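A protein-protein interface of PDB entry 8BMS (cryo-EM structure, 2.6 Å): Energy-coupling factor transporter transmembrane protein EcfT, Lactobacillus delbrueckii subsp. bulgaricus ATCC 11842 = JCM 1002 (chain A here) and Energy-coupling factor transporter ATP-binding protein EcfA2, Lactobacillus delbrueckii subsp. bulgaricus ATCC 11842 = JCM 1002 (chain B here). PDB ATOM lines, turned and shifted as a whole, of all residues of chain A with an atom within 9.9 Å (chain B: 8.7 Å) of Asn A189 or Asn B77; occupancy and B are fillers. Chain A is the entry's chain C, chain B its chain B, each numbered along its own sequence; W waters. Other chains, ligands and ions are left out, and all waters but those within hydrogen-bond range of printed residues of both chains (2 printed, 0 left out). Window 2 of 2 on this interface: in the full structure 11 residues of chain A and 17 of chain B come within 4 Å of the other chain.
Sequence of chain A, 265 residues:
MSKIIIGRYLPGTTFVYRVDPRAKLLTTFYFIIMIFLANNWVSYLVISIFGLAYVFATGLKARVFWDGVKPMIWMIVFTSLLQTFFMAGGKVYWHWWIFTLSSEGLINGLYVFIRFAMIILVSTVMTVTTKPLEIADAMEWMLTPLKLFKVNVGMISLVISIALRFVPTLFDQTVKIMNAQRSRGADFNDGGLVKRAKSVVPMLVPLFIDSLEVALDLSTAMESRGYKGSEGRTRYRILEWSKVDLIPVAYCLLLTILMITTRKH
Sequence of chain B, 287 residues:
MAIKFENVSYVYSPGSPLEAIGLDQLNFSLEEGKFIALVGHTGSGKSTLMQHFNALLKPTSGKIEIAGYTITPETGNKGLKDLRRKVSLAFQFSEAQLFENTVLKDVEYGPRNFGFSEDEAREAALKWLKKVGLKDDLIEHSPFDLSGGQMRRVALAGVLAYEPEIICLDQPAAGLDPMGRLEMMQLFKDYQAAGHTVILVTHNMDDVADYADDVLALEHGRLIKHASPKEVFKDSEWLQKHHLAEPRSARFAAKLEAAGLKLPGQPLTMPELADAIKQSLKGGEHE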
ATOM      1  N   VAL A 175      24.464   1.373 -25.444  1.00  0.00           N
ATOM      2  CA  VAL A 175      24.782   0.855 -26.772  1.00  0.00           C
ATOM      3  C   VAL A 175      26.175   1.301 -27.206  1.00  0.00           C
ATOM      4  O   VAL A 175      26.943   0.517 -27.777  1.00  0.00           O
ATOM      5  CB  VAL A 175      23.706   1.288 -27.785  1.00  0.00           C
ATOM      6  CG1 VAL A 175      24.125   0.919 -29.198  1.00  0.00           C
ATOM      7  CG2 VAL A 175      22.371   0.650 -27.438  1.00  0.00           C
ATOM      8  N   MET A 178      28.849  -0.536 -25.255  1.00  0.00           N
ATOM      9  CA  MET A 178      28.809  -1.945 -25.630  1.00  0.00           C
ATOM     10  C   MET A 178      29.470  -2.175 -26.985  1.00  0.00           C
ATOM     11  O   MET A 178      30.247  -3.120 -27.150  1.00  0.00           O
ATOM     12  CB  MET A 178      27.369  -2.456 -25.635  1.00  0.00           C
ATOM     13  CG  MET A 178      26.886  -2.940 -24.278  1.00  0.00           C
ATOM     14  SD  MET A 178      25.612  -4.210 -24.394  1.00  0.00           S
ATOM     15  CE  MET A 178      24.223  -3.243 -24.978  1.00  0.00           C
ATOM     16  N   ASN A 179      29.195  -1.304 -27.960  1.00  0.00           N
ATOM     17  CA  ASN A 179      29.843  -1.422 -29.264  1.00  0.00           C
ATOM     18  C   ASN A 179      31.343  -1.165 -29.168  1.00  0.00           C
ATOM     19  O   ASN A 179      32.141  -1.871 -29.797  1.00  0.00           O
ATOM     20  CB  ASN A 179      29.201  -0.456 -30.257  1.00  0.00           C
ATOM     21  CG  ASN A 179      27.904  -0.985 -30.828  1.00  0.00           C
ATOM     22  OD1 ASN A 179      27.733  -2.192 -30.999  1.00  0.00           O
ATOM     23  ND2 ASN A 179      26.978  -0.083 -31.127  1.00  0.00           N
ATOM     24  N   ARG A 182      32.879  -4.213 -27.621  1.00  0.00           N
ATOM     25  CA  ARG A 182      32.819  -5.340 -28.545  1.00  0.00           C
ATOM     26  C   ARG A 182      33.896  -5.231 -29.612  1.00  0.00           C
ATOM     27  O   ARG A 182      34.565  -6.219 -29.929  1.00  0.00           O
ATOM     28  CB  ARG A 182      31.440  -5.415 -29.197  1.00  0.00           C
ATOM     29  CG  ARG A 182      30.420  -6.230 -28.432  1.00  0.00           C
ATOM     30  CD  ARG A 182      29.022  -5.993 -28.975  1.00  0.00           C
ATOM     31  NE  ARG A 182      28.035  -6.835 -28.312  1.00  0.00           N
ATOM     32  CZ  ARG A 182      26.840  -6.418 -27.917  1.00  0.00           C
ATOM     33  NH1 ARG A 182      26.447  -5.170 -28.106  1.00  0.00           N
ATOM     34  NH2 ARG A 182      26.019  -7.276 -27.318  1.00  0.00           N
ATOM     35  N   SER A 183      34.085  -4.029 -30.165  1.00  0.00           N
ATOM     36  CA  SER A 183      35.071  -3.844 -31.224  1.00  0.00           C
ATOM     37  C   SER A 183      36.467  -4.252 -30.778  1.00  0.00           C
ATOM     38  O   SER A 183      37.258  -4.745 -31.590  1.00  0.00           O
ATOM     39  CB  SER A 183      35.074  -2.390 -31.690  1.00  0.00           C
ATOM     40  OG  SER A 183      33.801  -2.012 -32.180  1.00  0.00           O
ATOM     41  N   GLY A 185      37.155  -6.492 -28.282  1.00  0.00           N
ATOM     42  CA  GLY A 185      37.251  -7.864 -27.819  1.00  0.00           C
ATOM     43  C   GLY A 185      36.396  -8.252 -26.634  1.00  0.00           C
ATOM     44  O   GLY A 185      36.505  -9.395 -26.175  1.00  0.00           O
ATOM     45  N   ALA A 186      35.555  -7.364 -26.111  1.00  0.00           N
ATOM     46  CA  ALA A 186      34.682  -7.749 -25.012  1.00  0.00           C
ATOM     47  C   ALA A 186      33.618  -8.724 -25.497  1.00  0.00           C
ATOM     48  O   ALA A 186      33.130  -8.628 -26.626  1.00  0.00           O
ATOM     49  CB  ALA A 186      34.022  -6.523 -24.390  1.00  0.00           C
ATOM     50  N   ASP A 187      33.260  -9.673 -24.636  1.00  0.00           N
ATOM     51  CA  ASP A 187      32.254 -10.686 -24.947  1.00  0.00           C
ATOM     52  C   ASP A 187      31.184 -10.645 -23.861  1.00  0.00           C
ATOM     53  O   ASP A 187      31.361 -11.221 -22.784  1.00  0.00           O
ATOM     54  CB  ASP A 187      32.882 -12.071 -25.056  1.00  0.00           C
ATOM     55  CG  ASP A 187      32.186 -12.949 -26.076  1.00  0.00           C
ATOM     56  OD1 ASP A 187      30.947 -12.853 -26.198  1.00  0.00           O
ATOM     57  OD2 ASP A 187      32.875 -13.737 -26.754  1.00  0.00           O
ATOM     58  N   PHE A 188      30.079  -9.961 -24.144  1.00  0.00           N
ATOM     59  CA  PHE A 188      28.935  -9.920 -23.245  1.00  0.00           C
ATOM     60  C   PHE A 188      27.987 -11.093 -23.448  1.00  0.00           C
ATOM     61  O   PHE A 188      26.991 -11.200 -22.725  1.00  0.00           O
ATOM     62  CB  PHE A 188      28.167  -8.606 -23.419  1.00  0.00           C
ATOM     63  CG  PHE A 188      29.043  -7.387 -23.417  1.00  0.00           C
ATOM     64  CD1 PHE A 188      29.492  -6.844 -22.226  1.00  0.00           C
ATOM     65  CD2 PHE A 188      29.411  -6.782 -24.605  1.00  0.00           C
ATOM     66  CE1 PHE A 188      30.296  -5.722 -22.222  1.00  0.00           C
ATOM     67  CE2 PHE A 188      30.214  -5.660 -24.606  1.00  0.00           C
ATOM     68  CZ  PHE A 188      30.657  -5.129 -23.414  1.00  0.00           C
ATOM     69  N   ASN A 189      28.268 -11.966 -24.411  1.00  0.00           N
ATOM     70  CA  ASN A 189      27.425 -13.109 -24.732  1.00  0.00           C
ATOM     71  C   ASN A 189      28.187 -14.415 -24.552  1.00  0.00           C
ATOM     72  O   ASN A 189      28.131 -15.311 -25.397  1.00  0.00           O
ATOM     73  CB  ASN A 189      26.875 -12.995 -26.151  1.00  0.00           C
ATOM     74  CG  ASN A 189      25.850 -11.889 -26.290  1.00  0.00           C
ATOM     75  OD1 ASN A 189      24.997 -11.707 -25.422  1.00  0.00           O
ATOM     76  ND2 ASN A 189      25.930 -11.143 -27.382  1.00  0.00           N
ATOM     77  N   ASP A 190      28.917 -14.533 -23.447  1.00  0.00           N
ATOM     78  CA  ASP A 190      29.651 -15.744 -23.118  1.00  0.00           C
ATOM     79  C   ASP A 190      29.387 -16.122 -21.669  1.00  0.00           C
ATOM     80  O   ASP A 190      29.201 -15.258 -20.808  1.00  0.00           O
ATOM     81  CB  ASP A 190      31.158 -15.573 -23.347  1.00  0.00           C
ATOM     82  CG  ASP A 190      31.905 -16.892 -23.304  1.00  0.00           C
ATOM     83  OD1 ASP A 190      31.389 -17.886 -23.855  1.00  0.00           O
ATOM     84  OD2 ASP A 190      33.007 -16.935 -22.720  1.00  0.00           O
ATOM     85  N   GLY A 191      29.370 -17.426 -21.409  1.00  0.00           N
ATOM     86  CA  GLY A 191      29.178 -17.917 -20.063  1.00  0.00           C
ATOM     87  C   GLY A 191      27.737 -17.797 -19.593  1.00  0.00           C
ATOM     88  O   GLY A 191      26.820 -17.456 -20.342  1.00  0.00           O
ATOM     89  N   GLY A 192      27.555 -18.089 -18.309  1.00  0.00           N
ATOM     90  CA  GLY A 192      26.254 -18.012 -17.681  1.00  0.00           C
ATOM     91  C   GLY A 192      25.932 -16.608 -17.210  1.00  0.00           C
ATOM     92  O   GLY A 192      26.595 -15.627 -17.555  1.00  0.00           O
ATOM     93  N   LEU A 193      24.879 -16.519 -16.394  1.00  0.00           N
ATOM     94  CA  LEU A 193      24.449 -15.222 -15.881  1.00  0.00           C
ATOM     95  C   LEU A 193      25.519 -14.579 -15.011  1.00  0.00           C
ATOM     96  O   LEU A 193      25.682 -13.353 -15.034  1.00  0.00           O
ATOM     97  CB  LEU A 193      23.143 -15.363 -15.097  1.00  0.00           C
ATOM     98  CG  LEU A 193      21.819 -15.381 -15.870  1.00  0.00           C
ATOM     99  CD1 LEU A 193      21.595 -14.052 -16.580  1.00  0.00           C
ATOM    100  CD2 LEU A 193      21.727 -16.546 -16.852  1.00  0.00           C
ATOM    101  N   LYS A 195      28.825 -14.900 -15.321  1.00  0.00           N
ATOM    102  CA  LYS A 195      29.888 -14.377 -16.175  1.00  0.00           C
ATOM    103  C   LYS A 195      29.436 -13.132 -16.930  1.00  0.00           C
ATOM    104  O   LYS A 195      30.203 -12.173 -17.071  1.00  0.00           O
ATOM    105  CB  LYS A 195      30.358 -15.455 -17.151  1.00  0.00           C
ATOM    106  CG  LYS A 195      31.468 -14.992 -18.077  1.00  0.00           C
ATOM    107  CD  LYS A 195      32.749 -14.734 -17.302  1.00  0.00           C
ATOM    108  CE  LYS A 195      33.906 -14.420 -18.234  1.00  0.00           C
ATOM    109  NZ  LYS A 195      33.692 -13.130 -18.947  1.00  0.00           N
ATOM    110  N   ARG A 196      28.197 -13.125 -17.424  1.00  0.00           N
ATOM    111  CA  ARG A 196      27.693 -11.951 -18.129  1.00  0.00           C
ATOM    112  C   ARG A 196      27.557 -10.759 -17.189  1.00  0.00           C
ATOM    113  O   ARG A 196      27.875  -9.623 -17.565  1.00  0.00           O
ATOM    114  CB  ARG A 196      26.361 -12.282 -18.800  1.00  0.00           C
ATOM    115  CG  ARG A 196      26.468 -13.407 -19.820  1.00  0.00           C
ATOM    116  CD  ARG A 196      25.118 -13.793 -20.401  1.00  0.00           C
ATOM    117  NE  ARG A 196      24.607 -12.790 -21.327  1.00  0.00           N
ATOM    118  CZ  ARG A 196      23.427 -12.861 -21.928  1.00  0.00           C
ATOM    119  NH1 ARG A 196      22.606 -13.879 -21.723  1.00  0.00           N
ATOM    120  NH2 ARG A 196      23.060 -11.887 -22.756  1.00  0.00           N
ATOM    121  N   ALA A 197      27.092 -10.997 -15.959  1.00  0.00           N
ATOM    122  CA  ALA A 197      27.030  -9.924 -14.973  1.00  0.00           C
ATOM    123  C   ALA A 197      28.422  -9.400 -14.646  1.00  0.00           C
ATOM    124  O   ALA A 197      28.614  -8.190 -14.476  1.00  0.00           O
ATOM    125  CB  ALA A 197      26.326 -10.412 -13.708  1.00  0.00           C
ATOM    126  N   LYS A 198      29.405 -10.297 -14.549  1.00  0.00           N
ATOM    127  CA  LYS A 198      30.783  -9.869 -14.322  1.00  0.00           C
ATOM    128  C   LYS A 198      31.294  -9.022 -15.479  1.00  0.00           C
ATOM    129  O   LYS A 198      32.016  -8.041 -15.272  1.00  0.00           O
ATOM    130  CB  LYS A 198      31.678 -11.090 -14.116  1.00  0.00           C
ATOM    131  CG  LYS A 198      33.124 -10.761 -13.800  1.00  0.00           C
ATOM    132  CD  LYS A 198      33.954 -12.027 -13.668  1.00  0.00           C
ATOM    133  CE  LYS A 198      33.645 -12.754 -12.371  1.00  0.00           C
ATOM    134  NZ  LYS A 198      34.530 -13.935 -12.173  1.00  0.00           N
ATOM    135  N   SER A 199      30.940  -9.396 -16.709  1.00  0.00           N
ATOM    136  CA  SER A 199      31.384  -8.633 -17.871  1.00  0.00           C
ATOM    137  C   SER A 199      30.717  -7.265 -17.940  1.00  0.00           C
ATOM    138  O   SER A 199      31.335  -6.302 -18.409  1.00  0.00           O
ATOM    139  CB  SER A 199      31.112  -9.420 -19.153  1.00  0.00           C
ATOM    140  OG  SER A 199      29.734  -9.402 -19.480  1.00  0.00           O
ATOM    141  N   VAL A 200      29.463  -7.156 -17.492  1.00  0.00           N
ATOM    142  CA  VAL A 200      28.747  -5.884 -17.594  1.00  0.00           C
ATOM    143  C   VAL A 200      28.856  -5.012 -16.348  1.00  0.00           C
ATOM    144  O   VAL A 200      28.430  -3.848 -16.386  1.00  0.00           O
ATOM    145  CB  VAL A 200      27.253  -6.099 -17.908  1.00  0.00           C
ATOM    146  CG1 VAL A 200      27.086  -6.960 -19.149  1.00  0.00           C
ATOM    147  CG2 VAL A 200      26.540  -6.714 -16.715  1.00  0.00           C
ATOM    148  N   ASN B  54      33.538  -5.637 -39.374  1.00  0.00           N
ATOM    149  CA  ASN B  54      33.779  -6.332 -38.115  1.00  0.00           C
ATOM    150  C   ASN B  54      32.489  -6.790 -37.440  1.00  0.00           C
ATOM    151  O   ASN B  54      32.477  -7.030 -36.230  1.00  0.00           O
ATOM    152  CB  ASN B  54      34.596  -5.454 -37.166  1.00  0.00           C
ATOM    153  CG  ASN B  54      33.783  -4.333 -36.556  1.00  0.00           C
ATOM    154  OD1 ASN B  54      32.916  -3.752 -37.207  1.00  0.00           O
ATOM    155  ND2 ASN B  54      34.065  -4.019 -35.298  1.00  0.00           N
ATOM    156  N   ALA B  55      31.401  -6.908 -38.205  1.00  0.00           N
ATOM    157  CA  ALA B  55      30.137  -7.473 -37.734  1.00  0.00           C
ATOM    158  C   ALA B  55      29.516  -6.660 -36.602  1.00  0.00           C
ATOM    159  O   ALA B  55      28.762  -7.194 -35.786  1.00  0.00           O
ATOM    160  CB  ALA B  55      30.304  -8.935 -37.307  1.00  0.00           C
ATOM    161  N   LEU B  56      29.820  -5.362 -36.533  1.00  0.00           N
ATOM    162  CA  LEU B  56      29.062  -4.496 -35.638  1.00  0.00           C
ATOM    163  C   LEU B  56      27.638  -4.306 -36.139  1.00  0.00           C
ATOM    164  O   LEU B  56      26.716  -4.120 -35.336  1.00  0.00           O
ATOM    165  CB  LEU B  56      29.753  -3.142 -35.486  1.00  0.00           C
ATOM    166  CG  LEU B  56      30.956  -3.072 -34.544  1.00  0.00           C
ATOM    167  CD1 LEU B  56      31.345  -1.625 -34.298  1.00  0.00           C
ATOM    168  CD2 LEU B  56      30.663  -3.785 -33.234  1.00  0.00           C
ATOM    169  N   LEU B  57      27.444  -4.342 -37.453  1.00  0.00           N
ATOM    170  CA  LEU B  57      26.129  -4.337 -38.072  1.00  0.00           C
ATOM    171  C   LEU B  57      25.975  -5.616 -38.879  1.00  0.00           C
ATOM    172  O   LEU B  57      26.884  -5.996 -39.623  1.00  0.00           O
ATOM    173  CB  LEU B  57      25.943  -3.118 -38.982  1.00  0.00           C
ATOM    174  CG  LEU B  57      26.024  -1.721 -38.370  1.00  0.00           C
ATOM    175  CD1 LEU B  57      25.944  -0.664 -39.458  1.00  0.00           C
ATOM    176  CD2 LEU B  57      24.923  -1.518 -37.346  1.00  0.00           C
ATOM    177  N   LYS B  58      24.856  -6.269 -38.728  1.00  0.00           N
ATOM    178  CA  LYS B  58      24.718  -7.399 -39.630  1.00  0.00           C
ATOM    179  C   LYS B  58      23.988  -6.968 -40.897  1.00  0.00           C
ATOM    180  O   LYS B  58      23.099  -6.112 -40.847  1.00  0.00           O
ATOM    181  CB  LYS B  58      23.955  -8.534 -38.953  1.00  0.00           C
ATOM    182  CG  LYS B  58      24.368  -8.790 -37.514  1.00  0.00           C
ATOM    183  CD  LYS B  58      25.816  -9.243 -37.424  1.00  0.00           C
ATOM    184  CE  LYS B  58      26.227  -9.495 -35.985  1.00  0.00           C
ATOM    185  NZ  LYS B  58      25.986  -8.306 -35.122  1.00  0.00           N
ATOM    186  N   TYR B  69      35.393 -16.013 -41.377  1.00  0.00           N
ATOM    187  CA  TYR B  69      34.077 -15.824 -40.791  1.00  0.00           C
ATOM    188  C   TYR B  69      33.064 -15.554 -41.892  1.00  0.00           C
ATOM    189  O   TYR B  69      33.365 -14.859 -42.867  1.00  0.00           O
ATOM    190  CB  TYR B  69      34.073 -14.659 -39.797  1.00  0.00           C
ATOM    191  CG  TYR B  69      34.253 -15.065 -38.356  1.00  0.00           C
ATOM    192  CD1 TYR B  69      35.492 -15.457 -37.871  1.00  0.00           C
ATOM    193  CD2 TYR B  69      33.180 -15.049 -37.475  1.00  0.00           C
ATOM    194  CE1 TYR B  69      35.658 -15.828 -36.552  1.00  0.00           C
ATOM    195  CE2 TYR B  69      33.337 -15.416 -36.155  1.00  0.00           C
ATOM    196  CZ  TYR B  69      34.576 -15.804 -35.699  1.00  0.00           C
ATOM    197  OH  TYR B  69      34.731 -16.172 -34.384  1.00  0.00           O
ATOM    198  N   GLU B  74      21.431 -13.418 -40.295  1.00  0.00           N
ATOM    199  CA  GLU B  74      21.003 -14.113 -39.088  1.00  0.00           C
ATOM    200  C   GLU B  74      22.191 -14.703 -38.338  1.00  0.00           C
ATOM    201  O   GLU B  74      22.152 -15.866 -37.923  1.00  0.00           O
ATOM    202  CB  GLU B  74      20.001 -15.214 -39.441  1.00  0.00           C
ATOM    203  CG  GLU B  74      18.911 -14.773 -40.405  1.00  0.00           C
ATOM    204  CD  GLU B  74      19.222 -15.140 -41.844  1.00  0.00           C
ATOM    205  OE1 GLU B  74      20.330 -15.655 -42.102  1.00  0.00           O
ATOM    206  OE2 GLU B  74      18.358 -14.911 -42.716  1.00  0.00           O
ATOM    207  N   THR B  75      23.252 -13.916 -38.160  1.00  0.00           N
ATOM    208  CA  THR B  75      24.472 -14.414 -37.529  1.00  0.00           C
ATOM    209  C   THR B  75      24.410 -14.314 -36.006  1.00  0.00           C
ATOM    210  O   THR B  75      24.521 -15.325 -35.307  1.00  0.00           O
ATOM    211  CB  THR B  75      25.689 -13.655 -38.070  1.00  0.00           C
ATOM    212  OG1 THR B  75      25.956 -14.076 -39.413  1.00  0.00           O
ATOM    213  CG2 THR B  75      26.913 -13.932 -37.216  1.00  0.00           C
ATOM    214  N   GLY B  76      24.225 -13.106 -35.481  1.00  0.00           N
ATOM    215  CA  GLY B  76      24.195 -12.893 -34.050  1.00  0.00           C
ATOM    216  C   GLY B  76      25.558 -12.546 -33.476  1.00  0.00           C
ATOM    217  O   GLY B  76      26.605 -12.712 -34.106  1.00  0.00           O
ATOM    218  N   ASN B  77      25.534 -12.057 -32.236  1.00  0.00           N
ATOM    219  CA  ASN B  77      26.730 -11.559 -31.567  1.00  0.00           C
ATOM    220  C   ASN B  77      27.532 -12.648 -30.862  1.00  0.00           C
ATOM    221  O   ASN B  77      28.578 -12.338 -30.282  1.00  0.00           O
ATOM    222  CB  ASN B  77      26.349 -10.477 -30.553  1.00  0.00           C
ATOM    223  CG  ASN B  77      26.120  -9.127 -31.198  1.00  0.00           C
ATOM    224  OD1 ASN B  77      26.852  -8.728 -32.103  1.00  0.00           O
ATOM    225  ND2 ASN B  77      25.097  -8.418 -30.740  1.00  0.00           N
ATOM    226  N   LYS B  78      27.081 -13.896 -30.890  1.00  0.00           N
ATOM    227  CA  LYS B  78      27.779 -14.963 -30.188  1.00  0.00           C
ATOM    228  C   LYS B  78      28.941 -15.491 -31.019  1.00  0.00           C
ATOM    229  O   LYS B  78      28.817 -15.694 -32.229  1.00  0.00           O
ATOM    230  CB  LYS B  78      26.815 -16.102 -29.855  1.00  0.00           C
ATOM    231  CG  LYS B  78      27.433 -17.213 -29.024  1.00  0.00           C
ATOM    232  CD  LYS B  78      26.405 -18.270 -28.658  1.00  0.00           C
ATOM    233  CE  LYS B  78      27.032 -19.383 -27.833  1.00  0.00           C
ATOM    234  NZ  LYS B  78      26.040 -20.429 -27.467  1.00  0.00           N
ATOM    235  N   GLY B  79      30.076 -15.711 -30.358  1.00  0.00           N
ATOM    236  CA  GLY B  79      31.228 -16.289 -31.019  1.00  0.00           C
ATOM    237  C   GLY B  79      31.945 -15.372 -31.982  1.00  0.00           C
ATOM    238  O   GLY B  79      32.627 -15.857 -32.887  1.00  0.00           O
ATOM    239  N   LEU B  80      31.813 -14.059 -31.814  1.00  0.00           N
ATOM    240  CA  LEU B  80      32.416 -13.088 -32.717  1.00  0.00           C
ATOM    241  C   LEU B  80      33.698 -12.480 -32.165  1.00  0.00           C
ATOM    242  O   LEU B  80      34.194 -11.499 -32.725  1.00  0.00           O
ATOM    243  CB  LEU B  80      31.415 -11.977 -33.039  1.00  0.00           C
ATOM    244  CG  LEU B  80      30.301 -12.306 -34.031  1.00  0.00           C
ATOM    245  CD1 LEU B  80      29.412 -11.095 -34.243  1.00  0.00           C
ATOM    246  CD2 LEU B  80      30.884 -12.784 -35.348  1.00  0.00           C
ATOM    247  N   LYS B  81      34.248 -13.037 -31.085  1.00  0.00           N
ATOM    248  CA  LYS B  81      35.422 -12.427 -30.471  1.00  0.00           C
ATOM    249  C   LYS B  81      36.681 -12.663 -31.297  1.00  0.00           C
ATOM    250  O   LYS B  81      37.591 -11.827 -31.281  1.00  0.00           O
ATOM    251  CB  LYS B  81      35.612 -12.956 -29.050  1.00  0.00           C
ATOM    252  CG  LYS B  81      36.530 -12.097 -28.203  1.00  0.00           C
ATOM    253  CD  LYS B  81      37.134 -12.880 -27.055  1.00  0.00           C
ATOM    254  CE  LYS B  81      38.303 -12.128 -26.450  1.00  0.00           C
ATOM    255  NZ  LYS B  81      39.025 -12.936 -25.432  1.00  0.00           N
ATOM    256  N   ASP B  82      36.756 -13.778 -32.025  1.00  0.00           N
ATOM    257  CA  ASP B  82      37.940 -14.043 -32.839  1.00  0.00           C
ATOM    258  C   ASP B  82      37.943 -13.193 -34.105  1.00  0.00           C
ATOM    259  O   ASP B  82      39.007 -12.762 -34.571  1.00  0.00           O
ATOM    260  CB  ASP B  82      38.018 -15.529 -33.183  1.00  0.00           C
ATOM    261  CG  ASP B  82      39.445 -16.025 -33.304  1.00  0.00           C
ATOM    262  OD1 ASP B  82      40.296 -15.275 -33.826  1.00  0.00           O
ATOM    263  OD2 ASP B  82      39.718 -17.166 -32.875  1.00  0.00           O
ATOM    264  N   ARG B  84      36.831 -10.122 -34.332  1.00  0.00           N
ATOM    265  CA  ARG B  84      37.320  -8.824 -33.896  1.00  0.00           C
ATOM    266  C   ARG B  84      38.719  -8.903 -33.302  1.00  0.00           C
ATOM    267  O   ARG B  84      39.372  -7.865 -33.151  1.00  0.00           O
ATOM    268  CB  ARG B  84      36.325  -8.226 -32.905  1.00  0.00           C
ATOM    269  CG  ARG B  84      34.890  -8.423 -33.375  1.00  0.00           C
ATOM    270  CD  ARG B  84      33.894  -7.625 -32.573  1.00  0.00           C
ATOM    271  NE  ARG B  84      32.586  -7.582 -33.215  1.00  0.00           N
ATOM    272  CZ  ARG B  84      31.465  -8.005 -32.650  1.00  0.00           C
ATOM    273  NH1 ARG B  84      31.457  -8.528 -31.437  1.00  0.00           N
ATOM    274  NH2 ARG B  84      30.322  -7.905 -33.321  1.00  0.00           N
HETATM  275  O   HOH W   1      32.023  -9.786 -28.905  1.00  0.00           O
HETATM  276  O   HOH W   2      26.965  -4.782 -32.151  1.00  0.00           O
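Of the 16 printed residues of chain B, 5 touch a printed residue of chain A.
Printed residues of chain B that touch a printed residue of chain A: Asn B54, Leu B56, Asn B77, Lys B81 and Arg B84.
Hydrophobic or aromatic side chains of chain B that line the printed part of chain A: Leu B56.
Among the printed residues, no Asp or Glu carboxylate lies within 4 Å of a Lys or Arg side-chain nitrogen of the other chain.
The side-chain hydroxyl (OG) of Ser A183 lies within hydrogen-bond range of the backbone carbonyl oxygen (O) of Asn A179 (2.9 Å).
The side-chain amide oxygen of Asn A189 is in hydrogen-bond range of the guanidinium group of Arg A196 (3.3 Å).
NE of Arg B84 is in hydrogen-bond range of O of Asn B54.
OD1 of Asn B77 sits at hydrogen-bond distance from NZ of Lys B58.
The backbone NH (N) of Asn A189 lies close to the side-chain carboxylate (OD1) of Asp A187.
The guanidinium group (NH2) of Arg B84 is in hydrogen-bond range of the backbone carbonyl oxygen (O) of Ala B55 (3.0 Å).
Water W1 lies within hydrogen-bond range of O of Ala A186 and NH1 of Arg B84.
Water W2 lies within hydrogen-bond range of OD1 of Asn A179 (2.9 Å) and O of Leu B56 (3.3 Å).
Asn B77 touches just these residues of chain A: Arg A182 (3.7 Å) and Asn A189 (3.3 Å).
No residue of chain A comes within 4 Å of Gly B76.
Printed residues of chain A within 4 Å of Leu B56: Ser A183 (3.3 Å).
Of the printed residues of chain B, Gly A185 touches Lys B81.
Of the printed residues of chain B, Ser A183 touches Asn B54 (3.7 Å), Leu B56 (3.3 Å) and Arg B84 (3.8 Å).
Printed residues of chain A within 4 Å of Arg B84: Arg A182 (3.1 Å) and Ser A183 (3.8 Å).
Of the printed residues of chain A, Asn B54 touches Ser A183 (3.7 Å).
Val A200 touches none of the printed residues of chain B.
Phe A188 touches none of the printed residues of chain B.
The nearest residue of chain B that does not touch Asn A189 is Lys B78 (4.2 Å).
The nearest printed residue of chain A that does not touch Lys B81 is Ala A186 (5.1 Å).
Among the printed residues, merely in contact across the chains: Arg A182 with Arg B84 (3.1 Å), Ser A183 with Leu B56 (3.3 Å), Asn A189 with Asn B77 (3.3 Å), Gly A185 with Lys B81 (3.3 Å), Asp A187 with Lys B81 (3.7 Å), Ser A183 with Asn B54 (3.7 Å), Arg A182 with Asn B77 (3.7 Å) and Ser A183 with Arg B84 (3.8 Å).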
